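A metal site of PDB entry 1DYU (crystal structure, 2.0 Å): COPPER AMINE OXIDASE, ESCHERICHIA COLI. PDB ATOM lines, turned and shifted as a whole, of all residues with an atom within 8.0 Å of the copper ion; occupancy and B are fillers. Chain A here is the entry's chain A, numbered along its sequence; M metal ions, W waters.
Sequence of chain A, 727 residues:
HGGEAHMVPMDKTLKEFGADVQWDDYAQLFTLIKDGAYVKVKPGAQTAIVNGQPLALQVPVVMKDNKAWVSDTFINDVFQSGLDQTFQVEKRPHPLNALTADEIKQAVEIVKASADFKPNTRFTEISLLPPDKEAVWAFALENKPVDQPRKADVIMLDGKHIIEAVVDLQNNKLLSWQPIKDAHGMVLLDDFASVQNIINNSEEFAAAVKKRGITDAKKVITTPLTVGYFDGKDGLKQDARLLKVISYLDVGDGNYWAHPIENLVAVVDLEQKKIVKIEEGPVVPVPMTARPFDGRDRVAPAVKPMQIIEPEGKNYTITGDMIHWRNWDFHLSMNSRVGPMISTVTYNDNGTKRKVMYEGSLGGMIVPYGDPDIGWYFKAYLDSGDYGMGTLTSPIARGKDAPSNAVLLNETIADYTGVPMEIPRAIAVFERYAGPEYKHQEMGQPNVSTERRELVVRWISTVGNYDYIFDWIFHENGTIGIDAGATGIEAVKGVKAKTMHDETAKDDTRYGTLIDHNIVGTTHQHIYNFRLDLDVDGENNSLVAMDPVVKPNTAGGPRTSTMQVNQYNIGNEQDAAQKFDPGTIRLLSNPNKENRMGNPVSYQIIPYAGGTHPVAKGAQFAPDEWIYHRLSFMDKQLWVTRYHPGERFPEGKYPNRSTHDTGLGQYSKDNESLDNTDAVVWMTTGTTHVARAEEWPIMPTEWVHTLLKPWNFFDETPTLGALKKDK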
ATOM      1  N   VAL A 367      -9.838 -25.373 -23.044  1.00  0.00           N
ATOM      2  CA  VAL A 367     -10.561 -24.134 -23.223  1.00  0.00           C
ATOM      3  C   VAL A 367     -11.828 -24.444 -24.040  1.00  0.00           C
ATOM      4  O   VAL A 367     -11.833 -24.361 -25.261  1.00  0.00           O
ATOM      5  CB  VAL A 367      -9.731 -23.029 -23.872  1.00  0.00           C
ATOM      6  CG1 VAL A 367     -10.516 -21.730 -23.868  1.00  0.00           C
ATOM      7  CG2 VAL A 367      -8.374 -22.888 -23.185  1.00  0.00           C
ATOM      8  N   TYR A 369     -15.796 -23.805 -25.336  1.00  0.00           N
ATOM      9  CA  TYR A 369     -16.681 -22.703 -25.627  1.00  0.00           C
ATOM     10  C   TYR A 369     -18.149 -23.015 -25.361  1.00  0.00           C
ATOM     11  O   TYR A 369     -18.518 -24.195 -25.301  1.00  0.00           O
ATOM     12  CB  TYR A 369     -16.402 -22.187 -27.057  1.00  0.00           C
ATOM     13  CG  TYR A 369     -15.150 -21.305 -27.074  1.00  0.00           C
ATOM     14  CD1 TYR A 369     -13.890 -21.899 -27.033  1.00  0.00           C
ATOM     15  CD2 TYR A 369     -15.233 -19.921 -27.089  1.00  0.00           C
ATOM     16  CE1 TYR A 369     -12.726 -21.121 -27.016  1.00  0.00           C
ATOM     17  CE2 TYR A 369     -14.097 -19.139 -27.080  1.00  0.00           C
ATOM     18  CZ  TYR A 369     -12.846 -19.753 -27.043  1.00  0.00           C
ATOM     19  OH  TYR A 369     -11.728 -18.926 -27.026  1.00  0.00           O
ATOM     20  N   ASN A 465      -4.352 -18.055 -30.623  1.00  0.00           N
ATOM     21  CA  ASN A 465      -4.599 -16.738 -30.086  1.00  0.00           C
ATOM     22  C   ASN A 465      -4.309 -16.596 -28.590  1.00  0.00           C
ATOM     23  O   ASN A 465      -4.211 -15.457 -28.163  1.00  0.00           O
ATOM     24  CB  ASN A 465      -6.081 -16.340 -30.299  1.00  0.00           C
ATOM     25  CG  ASN A 465      -7.037 -17.388 -29.780  1.00  0.00           C
ATOM     26  OD1 ASN A 465      -6.831 -18.562 -30.004  1.00  0.00           O
ATOM     27  ND2 ASN A 465      -8.075 -16.900 -29.070  1.00  0.00           N
ATOM     28  N   TPQ A 466      -4.195 -17.643 -27.814  1.00  0.00           N
ATOM     29  CA  TPQ A 466      -3.944 -17.432 -26.363  1.00  0.00           C
ATOM     30  CB  TPQ A 466      -4.360 -18.628 -25.478  1.00  0.00           C
ATOM     31  C   TPQ A 466      -2.537 -17.634 -25.914  1.00  0.00           C
ATOM     32  O   TPQ A 466      -1.816 -18.439 -26.547  1.00  0.00           O
ATOM     33  C1  TPQ A 466      -5.720 -19.194 -25.933  1.00  0.00           C
ATOM     34  C2  TPQ A 466      -6.931 -18.483 -25.742  1.00  0.00           C
ATOM     35  O2  TPQ A 466      -6.932 -17.496 -25.236  1.00  0.00           O
ATOM     36  C3  TPQ A 466      -8.152 -19.002 -26.178  1.00  0.00           C
ATOM     37  C4  TPQ A 466      -8.185 -20.222 -26.833  1.00  0.00           C
ATOM     38  O4  TPQ A 466      -9.389 -20.743 -27.269  1.00  0.00           O
ATOM     39  C5  TPQ A 466      -7.010 -20.935 -27.036  1.00  0.00           C
ATOM     40  O5  TPQ A 466      -7.042 -21.912 -27.554  1.00  0.00           O
ATOM     41  C6  TPQ A 466      -5.806 -20.415 -26.600  1.00  0.00           C
ATOM     42  N   TYR A 468      -0.323 -18.313 -22.439  1.00  0.00           N
ATOM     43  CA  TYR A 468      -0.422 -18.780 -21.083  1.00  0.00           C
ATOM     44  C   TYR A 468       0.904 -18.656 -20.342  1.00  0.00           C
ATOM     45  O   TYR A 468       1.945 -19.029 -20.890  1.00  0.00           O
ATOM     46  CB  TYR A 468      -0.876 -20.234 -20.971  1.00  0.00           C
ATOM     47  CG  TYR A 468      -2.272 -20.363 -21.540  1.00  0.00           C
ATOM     48  CD1 TYR A 468      -3.353 -19.848 -20.850  1.00  0.00           C
ATOM     49  CD2 TYR A 468      -2.505 -20.965 -22.771  1.00  0.00           C
ATOM     50  CE1 TYR A 468      -4.631 -19.919 -21.355  1.00  0.00           C
ATOM     51  CE2 TYR A 468      -3.784 -21.043 -23.288  1.00  0.00           C
ATOM     52  CZ  TYR A 468      -4.841 -20.517 -22.582  1.00  0.00           C
ATOM     53  OH  TYR A 468      -6.119 -20.588 -23.086  1.00  0.00           O
ATOM     54  N   ALA A 486      -3.395 -15.886 -18.009  1.00  0.00           N
ATOM     55  CA  ALA A 486      -3.885 -15.960 -19.382  1.00  0.00           C
ATOM     56  C   ALA A 486      -3.957 -14.568 -20.002  1.00  0.00           C
ATOM     57  O   ALA A 486      -4.510 -13.627 -19.411  1.00  0.00           O
ATOM     58  CB  ALA A 486      -5.294 -16.553 -19.441  1.00  0.00           C
ATOM     59  N   THR A 487      -3.408 -14.424 -21.209  1.00  0.00           N
ATOM     60  CA  THR A 487      -3.428 -13.175 -21.963  1.00  0.00           C
ATOM     61  C   THR A 487      -3.567 -13.563 -23.441  1.00  0.00           C
ATOM     62  O   THR A 487      -3.922 -14.713 -23.826  1.00  0.00           O
ATOM     63  CB  THR A 487      -2.255 -12.231 -21.649  1.00  0.00           C
ATOM     64  OG1 THR A 487      -2.385 -11.026 -22.450  1.00  0.00           O
ATOM     65  CG2 THR A 487      -0.894 -12.897 -21.886  1.00  0.00           C
ATOM     66  N   ILE A 489      -5.138 -12.846 -27.511  1.00  0.00           N
ATOM     67  CA  ILE A 489      -6.264 -12.275 -28.263  1.00  0.00           C
ATOM     68  C   ILE A 489      -7.539 -13.110 -28.157  1.00  0.00           C
ATOM     69  O   ILE A 489      -7.563 -14.313 -28.355  1.00  0.00           O
ATOM     70  CB  ILE A 489      -5.870 -12.301 -29.770  1.00  0.00           C
ATOM     71  CG1 ILE A 489      -4.524 -11.603 -29.974  1.00  0.00           C
ATOM     72  CG2 ILE A 489      -7.014 -11.592 -30.511  1.00  0.00           C
ATOM     73  CD1 ILE A 489      -4.260 -10.248 -29.365  1.00  0.00           C
ATOM     74  N   GLU A 490      -8.677 -12.479 -27.835  1.00  0.00           N
ATOM     75  CA  GLU A 490      -9.895 -13.271 -27.742  1.00  0.00           C
ATOM     76  C   GLU A 490     -10.426 -13.831 -29.049  1.00  0.00           C
ATOM     77  O   GLU A 490     -10.341 -13.152 -30.068  1.00  0.00           O
ATOM     78  CB  GLU A 490     -10.978 -12.436 -27.058  1.00  0.00           C
ATOM     79  CG  GLU A 490     -10.904 -12.681 -25.542  1.00  0.00           C
ATOM     80  CD  GLU A 490     -11.878 -11.808 -24.774  1.00  0.00           C
ATOM     81  OE1 GLU A 490     -13.067 -11.718 -25.158  1.00  0.00           O
ATOM     82  OE2 GLU A 490     -11.421 -11.221 -23.764  1.00  0.00           O
ATOM     83  N   ALA A 491     -10.964 -15.062 -29.004  1.00  0.00           N
ATOM     84  CA  ALA A 491     -11.551 -15.699 -30.172  1.00  0.00           C
ATOM     85  C   ALA A 491     -12.892 -14.961 -30.283  1.00  0.00           C
ATOM     86  O   ALA A 491     -13.653 -15.067 -29.312  1.00  0.00           O
ATOM     87  CB  ALA A 491     -11.833 -17.172 -29.865  1.00  0.00           C
ATOM     88  N   THR A 522     -17.092 -14.556 -27.330  1.00  0.00           N
ATOM     89  CA  THR A 522     -17.790 -15.728 -26.889  1.00  0.00           C
ATOM     90  C   THR A 522     -17.343 -16.297 -25.547  1.00  0.00           C
ATOM     91  O   THR A 522     -16.162 -16.587 -25.260  1.00  0.00           O
ATOM     92  CB  THR A 522     -17.707 -16.837 -27.938  1.00  0.00           C
ATOM     93  OG1 THR A 522     -18.222 -16.309 -29.177  1.00  0.00           O
ATOM     94  CG2 THR A 522     -18.490 -18.042 -27.455  1.00  0.00           C
ATOM     95  N   THR A 523     -18.371 -16.500 -24.704  1.00  0.00           N
ATOM     96  CA  THR A 523     -18.122 -17.067 -23.390  1.00  0.00           C
ATOM     97  C   THR A 523     -17.441 -18.411 -23.476  1.00  0.00           C
ATOM     98  O   THR A 523     -17.761 -19.206 -24.358  1.00  0.00           O
ATOM     99  CB  THR A 523     -19.459 -17.177 -22.612  1.00  0.00           C
ATOM    100  OG1 THR A 523     -19.909 -15.810 -22.418  1.00  0.00           O
ATOM    101  CG2 THR A 523     -19.206 -17.672 -21.168  1.00  0.00           C
ATOM    102  N   HIS A 524     -16.511 -18.672 -22.571  1.00  0.00           N
ATOM    103  CA  HIS A 524     -15.828 -19.951 -22.538  1.00  0.00           C
ATOM    104  C   HIS A 524     -15.137 -20.094 -21.176  1.00  0.00           C
ATOM    105  O   HIS A 524     -15.242 -19.155 -20.396  1.00  0.00           O
ATOM    106  CB  HIS A 524     -14.766 -20.040 -23.673  1.00  0.00           C
ATOM    107  CG  HIS A 524     -13.795 -18.838 -23.560  1.00  0.00           C
ATOM    108  ND1 HIS A 524     -14.143 -17.575 -23.969  1.00  0.00           N
ATOM    109  CD2 HIS A 524     -12.549 -18.749 -23.055  1.00  0.00           C
ATOM    110  CE1 HIS A 524     -13.147 -16.746 -23.731  1.00  0.00           C
ATOM    111  NE2 HIS A 524     -12.170 -17.436 -23.170  1.00  0.00           N
ATOM    112  N   GLN A 525     -14.493 -21.216 -20.880  1.00  0.00           N
ATOM    113  CA  GLN A 525     -13.810 -21.373 -19.607  1.00  0.00           C
ATOM    114  C   GLN A 525     -12.339 -21.703 -19.933  1.00  0.00           C
ATOM    115  O   GLN A 525     -11.996 -22.111 -21.050  1.00  0.00           O
ATOM    116  CB  GLN A 525     -14.319 -22.665 -18.888  1.00  0.00           C
ATOM    117  CG  GLN A 525     -15.794 -22.519 -18.487  1.00  0.00           C
ATOM    118  CD  GLN A 525     -16.207 -23.644 -17.570  1.00  0.00           C
ATOM    119  OE1 GLN A 525     -16.182 -23.465 -16.347  1.00  0.00           O
ATOM    120  NE2 GLN A 525     -16.541 -24.756 -18.200  1.00  0.00           N
ATOM    121  N   HIS A 526     -11.494 -21.569 -18.941  1.00  0.00           N
ATOM    122  CA  HIS A 526     -10.068 -21.898 -19.018  1.00  0.00           C
ATOM    123  C   HIS A 526      -9.919 -22.903 -17.867  1.00  0.00           C
ATOM    124  O   HIS A 526     -10.095 -22.558 -16.677  1.00  0.00           O
ATOM    125  CB  HIS A 526      -9.093 -20.760 -18.762  1.00  0.00           C
ATOM    126  CG  HIS A 526      -9.079 -19.753 -19.909  1.00  0.00           C
ATOM    127  ND1 HIS A 526      -8.320 -19.941 -21.038  1.00  0.00           N
ATOM    128  CD2 HIS A 526      -9.723 -18.580 -20.063  1.00  0.00           C
ATOM    129  CE1 HIS A 526      -8.497 -18.929 -21.854  1.00  0.00           C
ATOM    130  NE2 HIS A 526      -9.347 -18.088 -21.290  1.00  0.00           N
ATOM    131  N   TYR A 528      -7.322 -25.566 -16.116  1.00  0.00           N
ATOM    132  CA  TYR A 528      -5.962 -26.058 -16.027  1.00  0.00           C
ATOM    133  C   TYR A 528      -5.929 -27.207 -15.030  1.00  0.00           C
ATOM    134  O   TYR A 528      -6.648 -27.118 -14.036  1.00  0.00           O
ATOM    135  CB  TYR A 528      -5.010 -24.978 -15.416  1.00  0.00           C
ATOM    136  CG  TYR A 528      -5.121 -23.624 -16.084  1.00  0.00           C
ATOM    137  CD1 TYR A 528      -4.493 -23.354 -17.297  1.00  0.00           C
ATOM    138  CD2 TYR A 528      -5.883 -22.622 -15.521  1.00  0.00           C
ATOM    139  CE1 TYR A 528      -4.586 -22.131 -17.915  1.00  0.00           C
ATOM    140  CE2 TYR A 528      -6.012 -21.366 -16.132  1.00  0.00           C
ATOM    141  CZ  TYR A 528      -5.362 -21.156 -17.336  1.00  0.00           C
ATOM    142  OH  TYR A 528      -5.488 -19.928 -17.930  1.00  0.00           O
ATOM    143  N   HIS A 613     -10.581 -13.602 -12.545  1.00  0.00           N
ATOM    144  CA  HIS A 613     -11.741 -13.740 -13.437  1.00  0.00           C
ATOM    145  C   HIS A 613     -12.733 -14.611 -12.642  1.00  0.00           C
ATOM    146  O   HIS A 613     -12.348 -15.297 -11.686  1.00  0.00           O
ATOM    147  CB  HIS A 613     -11.347 -14.547 -14.677  1.00  0.00           C
ATOM    148  CG  HIS A 613     -11.295 -13.745 -15.937  1.00  0.00           C
ATOM    149  ND1 HIS A 613     -10.821 -14.269 -17.135  1.00  0.00           N
ATOM    150  CD2 HIS A 613     -11.629 -12.460 -16.179  1.00  0.00           C
ATOM    151  CE1 HIS A 613     -10.880 -13.337 -18.069  1.00  0.00           C
ATOM    152  NE2 HIS A 613     -11.367 -12.233 -17.521  1.00  0.00           N
ATOM    153  N   THR A 687     -11.283 -20.746 -14.826  1.00  0.00           N
ATOM    154  CA  THR A 687     -12.071 -19.517 -14.755  1.00  0.00           C
ATOM    155  C   THR A 687     -13.242 -19.605 -15.734  1.00  0.00           C
ATOM    156  O   THR A 687     -13.183 -20.397 -16.670  1.00  0.00           O
ATOM    157  CB  THR A 687     -11.203 -18.337 -15.238  1.00  0.00           C
ATOM    158  OG1 THR A 687     -10.829 -18.438 -16.643  1.00  0.00           O
ATOM    159  CG2 THR A 687      -9.903 -18.238 -14.440  1.00  0.00           C
ATOM    160  N   THR A 688     -14.229 -18.786 -15.532  1.00  0.00           N
ATOM    161  CA  THR A 688     -15.355 -18.744 -16.467  1.00  0.00           C
ATOM    162  C   THR A 688     -15.136 -17.344 -17.055  1.00  0.00           C
ATOM    163  O   THR A 688     -15.214 -16.373 -16.296  1.00  0.00           O
ATOM    164  CB  THR A 688     -16.729 -18.864 -15.811  1.00  0.00           C
ATOM    165  OG1 THR A 688     -16.770 -20.230 -15.396  1.00  0.00           O
ATOM    166  CG2 THR A 688     -17.754 -18.614 -16.916  1.00  0.00           C
ATOM    167  N   HIS A 689     -14.869 -17.273 -18.355  1.00  0.00           N
ATOM    168  CA  HIS A 689     -14.626 -15.969 -18.955  1.00  0.00           C
ATOM    169  C   HIS A 689     -15.777 -15.317 -19.695  1.00  0.00           C
ATOM    170  O   HIS A 689     -16.127 -15.782 -20.776  1.00  0.00           O
ATOM    171  CB  HIS A 689     -13.380 -16.078 -19.861  1.00  0.00           C
ATOM    172  CG  HIS A 689     -12.883 -14.740 -20.434  1.00  0.00           C
ATOM    173  ND1 HIS A 689     -11.788 -14.659 -21.268  1.00  0.00           N
ATOM    174  CD2 HIS A 689     -13.334 -13.473 -20.279  1.00  0.00           C
ATOM    175  CE1 HIS A 689     -11.591 -13.403 -21.614  1.00  0.00           C
ATOM    176  NE2 HIS A 689     -12.511 -12.660 -21.028  1.00  0.00           N
ATOM    177  N   VAL A 690     -16.333 -14.261 -19.105  1.00  0.00           N
ATOM    178  CA  VAL A 690     -17.422 -13.530 -19.748  1.00  0.00           C
ATOM    179  C   VAL A 690     -16.651 -12.244 -20.113  1.00  0.00           C
ATOM    180  O   VAL A 690     -16.181 -11.553 -19.214  1.00  0.00           O
ATOM    181  CB  VAL A 690     -18.631 -13.262 -18.831  1.00  0.00           C
ATOM    182  CG1 VAL A 690     -19.637 -12.327 -19.508  1.00  0.00           C
ATOM    183  CG2 VAL A 690     -19.287 -14.604 -18.539  1.00  0.00           C
ATOM    184  N   ALA A 691     -16.510 -11.909 -21.378  1.00  0.00           N
ATOM    185  CA  ALA A 691     -15.778 -10.755 -21.844  1.00  0.00           C
ATOM    186  C   ALA A 691     -16.228  -9.338 -21.580  1.00  0.00           C
ATOM    187  O   ALA A 691     -17.359  -9.027 -21.211  1.00  0.00           O
ATOM    188  CB  ALA A 691     -15.513 -10.836 -23.351  1.00  0.00           C
ATOM    189  N   GLU A 695     -10.907  -5.938 -22.663  1.00  0.00           N
ATOM    190  CA  GLU A 695     -10.068  -7.027 -23.139  1.00  0.00           C
ATOM    191  C   GLU A 695      -9.860  -7.143 -24.645  1.00  0.00           C
ATOM    192  O   GLU A 695      -9.392  -8.160 -25.226  1.00  0.00           O
ATOM    193  CB  GLU A 695     -10.713  -8.333 -22.599  1.00  0.00           C
ATOM    194  CG  GLU A 695     -10.894  -8.419 -21.091  1.00  0.00           C
ATOM    195  CD  GLU A 695     -11.769  -9.562 -20.604  1.00  0.00           C
ATOM    196  OE1 GLU A 695     -12.598 -10.145 -21.335  1.00  0.00           O
ATOM    197  OE2 GLU A 695     -11.663 -10.014 -19.437  1.00  0.00           O
ATOM    198  N   MET A 699      -5.959  -8.789 -24.488  1.00  0.00           N
ATOM    199  CA  MET A 699      -6.366  -9.019 -23.100  1.00  0.00           C
ATOM    200  C   MET A 699      -5.382  -8.893 -21.974  1.00  0.00           C
ATOM    201  O   MET A 699      -4.330  -9.525 -21.904  1.00  0.00           O
ATOM    202  CB  MET A 699      -6.974 -10.441 -23.012  1.00  0.00           C
ATOM    203  CG  MET A 699      -7.210 -10.841 -21.563  1.00  0.00           C
ATOM    204  SD  MET A 699      -8.453 -12.134 -21.257  1.00  0.00           S
ATOM    205  CE  MET A 699      -7.577 -13.242 -20.141  1.00  0.00           C
ATOM    206  N   GLU A 702      -4.885 -12.270 -16.829  1.00  0.00           N
ATOM    207  CA  GLU A 702      -5.751 -12.625 -15.712  1.00  0.00           C
ATOM    208  C   GLU A 702      -5.071 -13.805 -15.006  1.00  0.00           C
ATOM    209  O   GLU A 702      -4.604 -14.737 -15.670  1.00  0.00           O
ATOM    210  CB  GLU A 702      -7.166 -13.021 -16.148  1.00  0.00           C
ATOM    211  CG  GLU A 702      -7.852 -11.934 -16.971  1.00  0.00           C
ATOM    212  CD  GLU A 702      -8.428 -10.852 -16.067  1.00  0.00           C
ATOM    213  OE1 GLU A 702      -8.270 -10.881 -14.830  1.00  0.00           O
ATOM    214  OE2 GLU A 702      -9.081  -9.937 -16.619  1.00  0.00           O
HETATM  215 CU    CU M   1     -10.638 -16.490 -21.800  1.00  0.00          CU
HETATM  216  O   HOH W   1      -9.497 -15.932 -24.418  1.00  0.00           O
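A ring nitrogen (NE2) of His 689 is in hydrogen-bond range of the side-chain carboxylate of Glu 695 (2.5 Å).
A ring nitrogen (ND1) of His 524 is in hydrogen-bond range of the backbone carbonyl oxygen (O) of Thr 522 (2.6 Å).
NE2 of His 689 lies close to OE2 of Glu 490, at 3.3 Å.
The side-chain hydroxyl (OH) of Tyr 468 sits at hydrogen-bond distance from a ring nitrogen (ND1) of His 526.
O of His 526 sits at hydrogen-bond distance from N of Thr 687.
Within 4 Å of the copper ion: His 524, His 526 and His 689.
The nearest printed residue that does not touch the copper ion is Met 699 (4.8 Å).
NE2 of His 526 binds the copper ion.
The copper ion is bound by ND1 of His 689, 2.2 Å away.
The copper ion is bound by a ring nitrogen (NE2) of His 524.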
